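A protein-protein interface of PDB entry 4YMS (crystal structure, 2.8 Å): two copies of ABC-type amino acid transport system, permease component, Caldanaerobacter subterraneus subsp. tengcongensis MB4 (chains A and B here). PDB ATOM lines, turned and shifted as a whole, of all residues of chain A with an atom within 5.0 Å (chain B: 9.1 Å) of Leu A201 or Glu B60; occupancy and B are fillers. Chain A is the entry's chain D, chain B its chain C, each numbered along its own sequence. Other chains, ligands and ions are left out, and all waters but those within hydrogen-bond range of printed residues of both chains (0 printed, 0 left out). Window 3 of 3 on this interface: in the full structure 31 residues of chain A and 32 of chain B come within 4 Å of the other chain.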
ATOM      1  N   TYR A 196     -22.734 -12.632   7.954  1.00  0.00           N
ATOM      2  CA  TYR A 196     -21.385 -12.071   8.145  1.00  0.00           C
ATOM      3  C   TYR A 196     -21.012 -11.171   6.964  1.00  0.00           C
ATOM      4  O   TYR A 196     -20.390 -10.123   7.142  1.00  0.00           O
ATOM      5  CB  TYR A 196     -20.332 -13.182   8.303  1.00  0.00           C
ATOM      6  CG  TYR A 196     -20.195 -13.741   9.708  1.00  0.00           C
ATOM      7  CD1 TYR A 196     -19.603 -13.002  10.715  1.00  0.00           C
ATOM      8  CD2 TYR A 196     -20.683 -15.014  10.024  1.00  0.00           C
ATOM      9  CE1 TYR A 196     -19.482 -13.512  12.003  1.00  0.00           C
ATOM     10  CE2 TYR A 196     -20.576 -15.539  11.313  1.00  0.00           C
ATOM     11  CZ  TYR A 196     -19.973 -14.784  12.305  1.00  0.00           C
ATOM     12  OH  TYR A 196     -19.857 -15.285  13.595  1.00  0.00           O
ATOM     13  N   PHE A 197     -21.394 -11.591   5.757  1.00  0.00           N
ATOM     14  CA  PHE A 197     -21.108 -10.825   4.550  1.00  0.00           C
ATOM     15  C   PHE A 197     -21.793  -9.478   4.598  1.00  0.00           C
ATOM     16  O   PHE A 197     -21.142  -8.444   4.450  1.00  0.00           O
ATOM     17  CB  PHE A 197     -21.561 -11.568   3.318  1.00  0.00           C
ATOM     18  CG  PHE A 197     -21.222 -10.870   2.026  1.00  0.00           C
ATOM     19  CD1 PHE A 197     -19.901 -10.761   1.604  1.00  0.00           C
ATOM     20  CD2 PHE A 197     -22.222 -10.355   1.213  1.00  0.00           C
ATOM     21  CE1 PHE A 197     -19.588 -10.146   0.408  1.00  0.00           C
ATOM     22  CE2 PHE A 197     -21.909  -9.742   0.011  1.00  0.00           C
ATOM     23  CZ  PHE A 197     -20.591  -9.639  -0.389  1.00  0.00           C
ATOM     24  N   VAL A 198     -23.105  -9.496   4.821  1.00  0.00           N
ATOM     25  CA  VAL A 198     -23.889  -8.268   4.903  1.00  0.00           C
ATOM     26  C   VAL A 198     -23.369  -7.336   6.005  1.00  0.00           C
ATOM     27  O   VAL A 198     -23.294  -6.115   5.825  1.00  0.00           O
ATOM     28  CB  VAL A 198     -25.383  -8.579   5.130  1.00  0.00           C
ATOM     29  CG1 VAL A 198     -26.106  -7.378   5.715  1.00  0.00           C
ATOM     30  CG2 VAL A 198     -26.024  -9.006   3.818  1.00  0.00           C
ATOM     31  N   MET A 199     -22.983  -7.912   7.133  1.00  0.00           N
ATOM     32  CA  MET A 199     -22.432  -7.115   8.226  1.00  0.00           C
ATOM     33  C   MET A 199     -21.126  -6.440   7.813  1.00  0.00           C
ATOM     34  O   MET A 199     -20.911  -5.247   8.068  1.00  0.00           O
ATOM     35  CB  MET A 199     -22.203  -7.978   9.458  1.00  0.00           C
ATOM     36  CG  MET A 199     -23.042  -7.590  10.644  1.00  0.00           C
ATOM     37  SD  MET A 199     -22.300  -8.258  12.146  1.00  0.00           S
ATOM     38  CE  MET A 199     -22.071  -9.977  11.654  1.00  0.00           C
ATOM     39  N   THR A 200     -20.259  -7.223   7.180  1.00  0.00           N
ATOM     40  CA  THR A 200     -18.974  -6.728   6.719  1.00  0.00           C
ATOM     41  C   THR A 200     -19.155  -5.590   5.712  1.00  0.00           C
ATOM     42  O   THR A 200     -18.527  -4.541   5.844  1.00  0.00           O
ATOM     43  CB  THR A 200     -18.132  -7.860   6.108  1.00  0.00           C
ATOM     44  OG1 THR A 200     -17.515  -8.601   7.171  1.00  0.00           O
ATOM     45  CG2 THR A 200     -17.034  -7.289   5.206  1.00  0.00           C
ATOM     46  N   LEU A 201     -20.028  -5.793   4.729  1.00  0.00           N
ATOM     47  CA  LEU A 201     -20.316  -4.759   3.750  1.00  0.00           C
ATOM     48  C   LEU A 201     -20.794  -3.489   4.421  1.00  0.00           C
ATOM     49  O   LEU A 201     -20.254  -2.399   4.182  1.00  0.00           O
ATOM     50  CB  LEU A 201     -21.372  -5.215   2.753  1.00  0.00           C
ATOM     51  CG  LEU A 201     -20.901  -6.123   1.629  1.00  0.00           C
ATOM     52  CD1 LEU A 201     -21.928  -6.094   0.519  1.00  0.00           C
ATOM     53  CD2 LEU A 201     -19.528  -5.733   1.125  1.00  0.00           C
ATOM     54  N   THR A 202     -21.808  -3.634   5.259  1.00  0.00           N
ATOM     55  CA  THR A 202     -22.354  -2.489   5.962  1.00  0.00           C
ATOM     56  C   THR A 202     -21.258  -1.677   6.658  1.00  0.00           C
ATOM     57  O   THR A 202     -21.063  -0.476   6.366  1.00  0.00           O
ATOM     58  CB  THR A 202     -23.406  -2.952   6.978  1.00  0.00           C
ATOM     59  OG1 THR A 202     -24.507  -3.520   6.258  1.00  0.00           O
ATOM     60  CG2 THR A 202     -23.906  -1.791   7.834  1.00  0.00           C
ATOM     61  N   PHE A 203     -20.511  -2.345   7.535  1.00  0.00           N
ATOM     62  CA  PHE A 203     -19.484  -1.659   8.316  1.00  0.00           C
ATOM     63  C   PHE A 203     -18.332  -1.078   7.475  1.00  0.00           C
ATOM     64  O   PHE A 203     -17.783  -0.029   7.825  1.00  0.00           O
ATOM     65  CB  PHE A 203     -18.934  -2.600   9.382  1.00  0.00           C
ATOM     66  CG  PHE A 203     -19.833  -2.741  10.584  1.00  0.00           C
ATOM     67  CD1 PHE A 203     -20.223  -1.625  11.305  1.00  0.00           C
ATOM     68  CD2 PHE A 203     -20.283  -3.992  10.997  1.00  0.00           C
ATOM     69  CE1 PHE A 203     -21.045  -1.750  12.414  1.00  0.00           C
ATOM     70  CE2 PHE A 203     -21.103  -4.118  12.105  1.00  0.00           C
ATOM     71  CZ  PHE A 203     -21.483  -2.995  12.815  1.00  0.00           C
ATOM     72  N   SER A 204     -17.986  -1.736   6.369  1.00  0.00           N
ATOM     73  CA  SER A 204     -16.954  -1.222   5.473  1.00  0.00           C
ATOM     74  C   SER A 204     -17.409   0.094   4.855  1.00  0.00           C
ATOM     75  O   SER A 204     -16.651   1.080   4.792  1.00  0.00           O
ATOM     76  CB  SER A 204     -16.639  -2.227   4.361  1.00  0.00           C
ATOM     77  OG  SER A 204     -15.693  -3.191   4.777  1.00  0.00           O
ATOM     78  N   LYS A 205     -18.662   0.089   4.405  1.00  0.00           N
ATOM     79  CA  LYS A 205     -19.288   1.273   3.843  1.00  0.00           C
ATOM     80  C   LYS A 205     -19.215   2.431   4.835  1.00  0.00           C
ATOM     81  O   LYS A 205     -18.596   3.469   4.530  1.00  0.00           O
ATOM     82  CB  LYS A 205     -20.736   0.968   3.438  1.00  0.00           C
ATOM     83  CG  LYS A 205     -21.605   2.178   3.116  1.00  0.00           C
ATOM     84  CD  LYS A 205     -22.973   2.094   3.811  1.00  0.00           C
ATOM     85  CE  LYS A 205     -23.892   1.055   3.132  1.00  0.00           C
ATOM     86  NZ  LYS A 205     -25.304   1.080   3.636  1.00  0.00           N
ATOM     87  N   ILE B  40      -8.238 -16.521 -10.491  1.00  0.00           N
ATOM     88  CA  ILE B  40      -9.322 -15.605 -10.158  1.00  0.00           C
ATOM     89  C   ILE B  40      -8.963 -14.210 -10.643  1.00  0.00           C
ATOM     90  O   ILE B  40      -9.815 -13.474 -11.145  1.00  0.00           O
ATOM     91  CB  ILE B  40      -9.590 -15.557  -8.627  1.00  0.00           C
ATOM     92  CG1 ILE B  40      -9.911 -16.950  -8.090  1.00  0.00           C
ATOM     93  CG2 ILE B  40     -10.715 -14.565  -8.290  1.00  0.00           C
ATOM     94  CD1 ILE B  40     -11.242 -17.450  -8.527  1.00  0.00           C
ATOM     95  N   LYS B  44     -10.757 -11.174 -13.204  1.00  0.00           N
ATOM     96  CA  LYS B  44     -11.147  -9.825 -12.820  1.00  0.00           C
ATOM     97  C   LYS B  44     -10.642  -8.795 -13.844  1.00  0.00           C
ATOM     98  O   LYS B  44     -11.140  -7.667 -13.915  1.00  0.00           O
ATOM     99  CB  LYS B  44     -10.612  -9.510 -11.425  1.00  0.00           C
ATOM    100  CG  LYS B  44     -11.385  -8.442 -10.692  1.00  0.00           C
ATOM    101  CD  LYS B  44     -10.746  -8.157  -9.348  1.00  0.00           C
ATOM    102  CE  LYS B  44     -11.591  -7.199  -8.527  1.00  0.00           C
ATOM    103  NZ  LYS B  44     -11.140  -7.140  -7.096  1.00  0.00           N
ATOM    104  N   LYS B  52     -15.910 -10.915 -14.737  1.00  0.00           N
ATOM    105  CA  LYS B  52     -15.426  -9.935 -13.775  1.00  0.00           C
ATOM    106  C   LYS B  52     -16.374  -9.826 -12.580  1.00  0.00           C
ATOM    107  O   LYS B  52     -15.925  -9.676 -11.437  1.00  0.00           O
ATOM    108  CB  LYS B  52     -15.236  -8.565 -14.445  1.00  0.00           C
ATOM    109  N   LEU B  53     -17.678  -9.866 -12.851  1.00  0.00           N
ATOM    110  CA  LEU B  53     -18.686  -9.805 -11.785  1.00  0.00           C
ATOM    111  C   LEU B  53     -18.607 -10.992 -10.832  1.00  0.00           C
ATOM    112  O   LEU B  53     -18.742 -10.847  -9.603  1.00  0.00           O
ATOM    113  CB  LEU B  53     -20.094  -9.723 -12.382  1.00  0.00           C
ATOM    114  CG  LEU B  53     -21.251  -9.765 -11.376  1.00  0.00           C
ATOM    115  CD1 LEU B  53     -21.261  -8.540 -10.466  1.00  0.00           C
ATOM    116  CD2 LEU B  53     -22.588  -9.910 -12.111  1.00  0.00           C
ATOM    117  N   VAL B  54     -18.398 -12.165 -11.422  1.00  0.00           N
ATOM    118  CA  VAL B  54     -18.297 -13.405 -10.667  1.00  0.00           C
ATOM    119  C   VAL B  54     -17.052 -13.383  -9.790  1.00  0.00           C
ATOM    120  O   VAL B  54     -17.124 -13.660  -8.598  1.00  0.00           O
ATOM    121  CB  VAL B  54     -18.245 -14.637 -11.606  1.00  0.00           C
ATOM    122  CG1 VAL B  54     -18.002 -15.909 -10.809  1.00  0.00           C
ATOM    123  CG2 VAL B  54     -19.527 -14.749 -12.417  1.00  0.00           C
ATOM    124  N   ALA B  55     -15.917 -13.017 -10.380  1.00  0.00           N
ATOM    125  CA  ALA B  55     -14.663 -12.989  -9.635  1.00  0.00           C
ATOM    126  C   ALA B  55     -14.710 -11.936  -8.528  1.00  0.00           C
ATOM    127  O   ALA B  55     -14.194 -12.148  -7.431  1.00  0.00           O
ATOM    128  CB  ALA B  55     -13.499 -12.739 -10.568  1.00  0.00           C
ATOM    129  N   SER B  56     -15.311 -10.792  -8.827  1.00  0.00           N
ATOM    130  CA  SER B  56     -15.447  -9.729  -7.844  1.00  0.00           C
ATOM    131  C   SER B  56     -16.326 -10.175  -6.679  1.00  0.00           C
ATOM    132  O   SER B  56     -15.995  -9.962  -5.505  1.00  0.00           O
ATOM    133  CB  SER B  56     -16.026  -8.480  -8.502  1.00  0.00           C
ATOM    134  OG  SER B  56     -15.115  -7.965  -9.456  1.00  0.00           O
ATOM    135  N   SER B  57     -17.442 -10.818  -7.010  1.00  0.00           N
ATOM    136  CA  SER B  57     -18.378 -11.293  -5.991  1.00  0.00           C
ATOM    137  C   SER B  57     -17.728 -12.377  -5.145  1.00  0.00           C
ATOM    138  O   SER B  57     -17.847 -12.374  -3.927  1.00  0.00           O
ATOM    139  CB  SER B  57     -19.660 -11.810  -6.637  1.00  0.00           C
ATOM    140  OG  SER B  57     -20.411 -10.742  -7.191  1.00  0.00           O
ATOM    141  N   TYR B  58     -17.043 -13.302  -5.810  1.00  0.00           N
ATOM    142  CA  TYR B  58     -16.260 -14.341  -5.159  1.00  0.00           C
ATOM    143  C   TYR B  58     -15.344 -13.753  -4.107  1.00  0.00           C
ATOM    144  O   TYR B  58     -15.531 -13.987  -2.903  1.00  0.00           O
ATOM    145  CB  TYR B  58     -15.445 -15.107  -6.205  1.00  0.00           C
ATOM    146  CG  TYR B  58     -14.508 -16.182  -5.671  1.00  0.00           C
ATOM    147  CD1 TYR B  58     -14.940 -17.499  -5.509  1.00  0.00           C
ATOM    148  CD2 TYR B  58     -13.185 -15.888  -5.354  1.00  0.00           C
ATOM    149  CE1 TYR B  58     -14.086 -18.485  -5.040  1.00  0.00           C
ATOM    150  CE2 TYR B  58     -12.320 -16.870  -4.887  1.00  0.00           C
ATOM    151  CZ  TYR B  58     -12.776 -18.169  -4.738  1.00  0.00           C
ATOM    152  OH  TYR B  58     -11.926 -19.144  -4.262  1.00  0.00           O
ATOM    153  N   ILE B  59     -14.392 -12.944  -4.576  1.00  0.00           N
ATOM    154  CA  ILE B  59     -13.376 -12.332  -3.721  1.00  0.00           C
ATOM    155  C   ILE B  59     -13.989 -11.564  -2.558  1.00  0.00           C
ATOM    156  O   ILE B  59     -13.573 -11.731  -1.408  1.00  0.00           O
ATOM    157  CB  ILE B  59     -12.474 -11.403  -4.529  1.00  0.00           C
ATOM    158  CG1 ILE B  59     -11.685 -12.214  -5.558  1.00  0.00           C
ATOM    159  CG2 ILE B  59     -11.526 -10.657  -3.611  1.00  0.00           C
ATOM    160  CD1 ILE B  59     -10.891 -11.373  -6.532  1.00  0.00           C
ATOM    161  N   GLU B  60     -14.977 -10.732  -2.866  1.00  0.00           N
ATOM    162  CA  GLU B  60     -15.649  -9.921  -1.856  1.00  0.00           C
ATOM    163  C   GLU B  60     -16.321 -10.801  -0.773  1.00  0.00           C
ATOM    164  O   GLU B  60     -16.249 -10.499   0.437  1.00  0.00           O
ATOM    165  CB  GLU B  60     -16.661  -8.990  -2.531  1.00  0.00           C
ATOM    166  CG  GLU B  60     -16.966  -7.717  -1.739  1.00  0.00           C
ATOM    167  CD  GLU B  60     -17.597  -6.631  -2.601  1.00  0.00           C
ATOM    168  OE1 GLU B  60     -18.119  -6.965  -3.693  1.00  0.00           O
ATOM    169  OE2 GLU B  60     -17.572  -5.450  -2.187  1.00  0.00           O
ATOM    170  N   VAL B  61     -16.972 -11.885  -1.219  1.00  0.00           N
ATOM    171  CA  VAL B  61     -17.672 -12.829  -0.326  1.00  0.00           C
ATOM    172  C   VAL B  61     -16.724 -13.599   0.583  1.00  0.00           C
ATOM    173  O   VAL B  61     -16.938 -13.658   1.785  1.00  0.00           O
ATOM    174  CB  VAL B  61     -18.517 -13.853  -1.127  1.00  0.00           C
ATOM    175  CG1 VAL B  61     -18.816 -15.085  -0.298  1.00  0.00           C
ATOM    176  CG2 VAL B  61     -19.802 -13.210  -1.628  1.00  0.00           C
ATOM    177  N   ILE B  62     -15.668 -14.163   0.007  1.00  0.00           N
ATOM    178  CA  ILE B  62     -14.686 -14.886   0.799  1.00  0.00           C
ATOM    179  C   ILE B  62     -13.922 -13.999   1.781  1.00  0.00           C
ATOM    180  O   ILE B  62     -13.720 -14.380   2.931  1.00  0.00           O
ATOM    181  CB  ILE B  62     -13.706 -15.593  -0.112  1.00  0.00           C
ATOM    182  CG1 ILE B  62     -14.439 -16.735  -0.788  1.00  0.00           C
ATOM    183  CG2 ILE B  62     -12.516 -16.136   0.667  1.00  0.00           C
ATOM    184  CD1 ILE B  62     -13.635 -17.411  -1.794  1.00  0.00           C
ATOM    185  N   ARG B  63     -13.519 -12.805   1.350  1.00  0.00           N
ATOM    186  CA  ARG B  63     -12.758 -11.926   2.231  1.00  0.00           C
ATOM    187  C   ARG B  63     -13.636 -11.358   3.324  1.00  0.00           C
ATOM    188  O   ARG B  63     -13.158 -11.051   4.413  1.00  0.00           O
ATOM    189  CB  ARG B  63     -12.106 -10.782   1.443  1.00  0.00           C
ATOM    190  CG  ARG B  63     -10.987 -11.213   0.506  1.00  0.00           C
ATOM    191  CD  ARG B  63     -10.332 -10.022  -0.214  1.00  0.00           C
ATOM    192  NE  ARG B  63      -9.734  -9.050   0.699  1.00  0.00           N
ATOM    193  CZ  ARG B  63      -9.900  -7.731   0.618  1.00  0.00           C
ATOM    194  NH1 ARG B  63     -10.635  -7.216  -0.365  1.00  0.00           N
ATOM    195  NH2 ARG B  63      -9.315  -6.930   1.510  1.00  0.00           N
ATOM    196  N   GLY B  64     -14.925 -11.227   3.032  1.00  0.00           N
ATOM    197  CA  GLY B  64     -15.847 -10.605   3.965  1.00  0.00           C
ATOM    198  C   GLY B  64     -16.529 -11.610   4.875  1.00  0.00           C
ATOM    199  O   GLY B  64     -17.506 -11.287   5.563  1.00  0.00           O
ATOM    200  N   THR B  65     -15.992 -12.829   4.903  1.00  0.00           N
ATOM    201  CA  THR B  65     -16.643 -13.946   5.585  1.00  0.00           C
ATOM    202  C   THR B  65     -15.604 -14.835   6.291  1.00  0.00           C
ATOM    203  O   THR B  65     -14.483 -14.999   5.796  1.00  0.00           O
ATOM    204  CB  THR B  65     -17.491 -14.738   4.559  1.00  0.00           C
ATOM    205  OG1 THR B  65     -18.861 -14.751   4.969  1.00  0.00           O
ATOM    206  CG2 THR B  65     -16.954 -16.148   4.302  1.00  0.00           C
ATOM    207  N   PRO B  66     -15.954 -15.373   7.476  1.00  0.00           N
ATOM    208  CA  PRO B  66     -14.948 -16.047   8.316  1.00  0.00           C
ATOM    209  C   PRO B  66     -14.355 -17.320   7.713  1.00  0.00           C
ATOM    210  O   PRO B  66     -15.006 -17.978   6.908  1.00  0.00           O
ATOM    211  CB  PRO B  66     -15.719 -16.359   9.605  1.00  0.00           C
ATOM    212  CG  PRO B  66     -16.860 -15.386   9.624  1.00  0.00           C
ATOM    213  CD  PRO B  66     -17.248 -15.248   8.174  1.00  0.00           C
ATOM    214  N   GLN B  70     -16.327 -21.159   6.541  1.00  0.00           N
ATOM    215  CA  GLN B  70     -16.009 -21.808   5.263  1.00  0.00           C
ATOM    216  C   GLN B  70     -15.594 -23.264   5.490  1.00  0.00           C
ATOM    217  O   GLN B  70     -15.982 -24.165   4.720  1.00  0.00           O
ATOM    218  CB  GLN B  70     -14.907 -21.048   4.527  1.00  0.00           C
ATOM    219  CG  GLN B  70     -15.321 -19.642   4.137  1.00  0.00           C
ATOM    220  CD  GLN B  70     -14.138 -18.721   3.843  1.00  0.00           C
ATOM    221  OE1 GLN B  70     -14.179 -17.531   4.164  1.00  0.00           O
ATOM    222  NE2 GLN B  70     -13.088 -19.266   3.222  1.00  0.00           N
ATOM    223  N   ALA B 101      -8.587 -16.138  -2.654  1.00  0.00           N
ATOM    224  CA  ALA B 101      -9.126 -14.788  -2.788  1.00  0.00           C
ATOM    225  C   ALA B 101      -8.041 -13.756  -2.479  1.00  0.00           C
ATOM    226  O   ALA B 101      -7.720 -12.869  -3.321  1.00  0.00           O
ATOM    227  CB  ALA B 101     -10.318 -14.582  -1.881  1.00  0.00           C
ATOM    228  N   TYR B 102      -7.434 -13.896  -1.297  1.00  0.00           N
ATOM    229  CA  TYR B 102      -6.439 -12.896  -0.887  1.00  0.00           C
ATOM    230  C   TYR B 102      -5.255 -12.799  -1.866  1.00  0.00           C
ATOM    231  O   TYR B 102      -4.698 -11.710  -2.074  1.00  0.00           O
ATOM    232  CB  TYR B 102      -5.932 -13.177   0.530  1.00  0.00           C
ATOM    233  CG  TYR B 102      -6.961 -12.854   1.585  1.00  0.00           C
ATOM    234  CD1 TYR B 102      -7.163 -11.552   2.006  1.00  0.00           C
ATOM    235  CD2 TYR B 102      -7.737 -13.855   2.158  1.00  0.00           C
ATOM    236  CE1 TYR B 102      -8.115 -11.248   2.976  1.00  0.00           C
ATOM    237  CE2 TYR B 102      -8.690 -13.559   3.125  1.00  0.00           C
ATOM    238  CZ  TYR B 102      -8.872 -12.256   3.531  1.00  0.00           C
ATOM    239  OH  TYR B 102      -9.821 -11.966   4.483  1.00  0.00           O
ATOM    240  N   ALA B 104      -5.462 -13.350  -5.134  1.00  0.00           N
ATOM    241  CA  ALA B 104      -5.979 -12.597  -6.287  1.00  0.00           C
ATOM    242  C   ALA B 104      -5.857 -11.074  -6.076  1.00  0.00           C
ATOM    243  O   ALA B 104      -5.382 -10.328  -6.972  1.00  0.00           O
ATOM    244  CB  ALA B 104      -7.432 -12.991  -6.573  1.00  0.00           C
ATOM    245  N   GLU B 105      -6.280 -10.628  -4.891  1.00  0.00           N
ATOM    246  CA  GLU B 105      -6.153  -9.209  -4.521  1.00  0.00           C
ATOM    247  C   GLU B 105      -4.698  -8.719  -4.457  1.00  0.00           C
ATOM    248  O   GLU B 105      -4.394  -7.599  -4.871  1.00  0.00           O
ATOM    249  CB  GLU B 105      -6.823  -8.946  -3.173  1.00  0.00           C
ATOM    250  CG  GLU B 105      -8.168  -8.253  -3.286  1.00  0.00           C
ATOM    251  CD  GLU B 105      -8.150  -7.149  -4.323  1.00  0.00           C
ATOM    252  OE1 GLU B 105      -7.525  -6.096  -4.048  1.00  0.00           O
ATOM    253  OE2 GLU B 105      -8.742  -7.347  -5.415  1.00  0.00           O
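The side-chain amide oxygen (OE1) of Gln B70 sits close to the backbone carbonyl oxygen (O) of Thr B65 (3.0 Å).
O of Pro B66 lies close to OE1 of Gln B70 (2.9 Å).
O of Tyr A196 sits at hydrogen-bond distance from OG1 of Thr A200 (3.3 Å).
The side-chain hydroxyl (OG) of Ser A204 sits at hydrogen-bond distance from the backbone carbonyl oxygen (O) of Thr A200 (3.3 Å).
Of the printed residues of chain B, Tyr A196 touches Gly B64, Thr B65 and Pro B66.
Of the printed residues of chain B, Phe A197 touches Glu B60 (3.4 Å), Val B61 (3.4 Å) and Gly B64 (3.8 Å).
Of chain B, only Gly B64 (3.1 Å) comes within 4 Å of Thr A200.
Of chain B, only Glu B60 (3.9 Å) comes within 4 Å of Leu A201.
Glu B60 touches just these residues of chain A: Phe A197 (3.4 Å) and Leu A201 (3.9 Å).
Printed residues of chain A within 4 Å of Val B61: Phe A197 (3.4 Å).
The nearest printed residue of chain B that does not touch Tyr A196 is Val B61 (7.0 Å).
No position is printed for both chains.
Of the 8 pairs that touch across the chains among the printed residues, none has its exchanged pair printed and touching as well.
The side-chain hydroxyl (OG1) of Thr A200 lies within hydrogen-bond range of the backbone carbonyl oxygen (O) of Gly B64 (3.1 Å).
The backbone carbonyl oxygen (O) of Tyr A196 lies close to the backbone carbonyl oxygen (O) of Gly B64 (3.5 Å).
OG1 of Thr B65 touches CB of Tyr A196, 3.97 Å away.
CG of Tyr A196 touches CD of Pro B66, at 3.6 Å.
Glu B60 touches Phe A197.
CA of Val B61 touches CE1 of Phe A197 (3.4 Å).
CA of Phe A197 touches O of Gly B64 (3.8 Å).
OE2 of Glu B60 touches CD2 of Leu A201 (3.9 Å).
Hydrophobic or aromatic side chains of chain B that line the printed part of chain A: Val B61 and Pro B66.
Printed residues of chain A that touch a printed residue of chain B: Tyr A196, Phe A197, Thr A200 and Leu A201.
Among the printed residues, no Asp or Glu carboxylate lies within 4 Å of a Lys or Arg side-chain nitrogen of the other chain.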
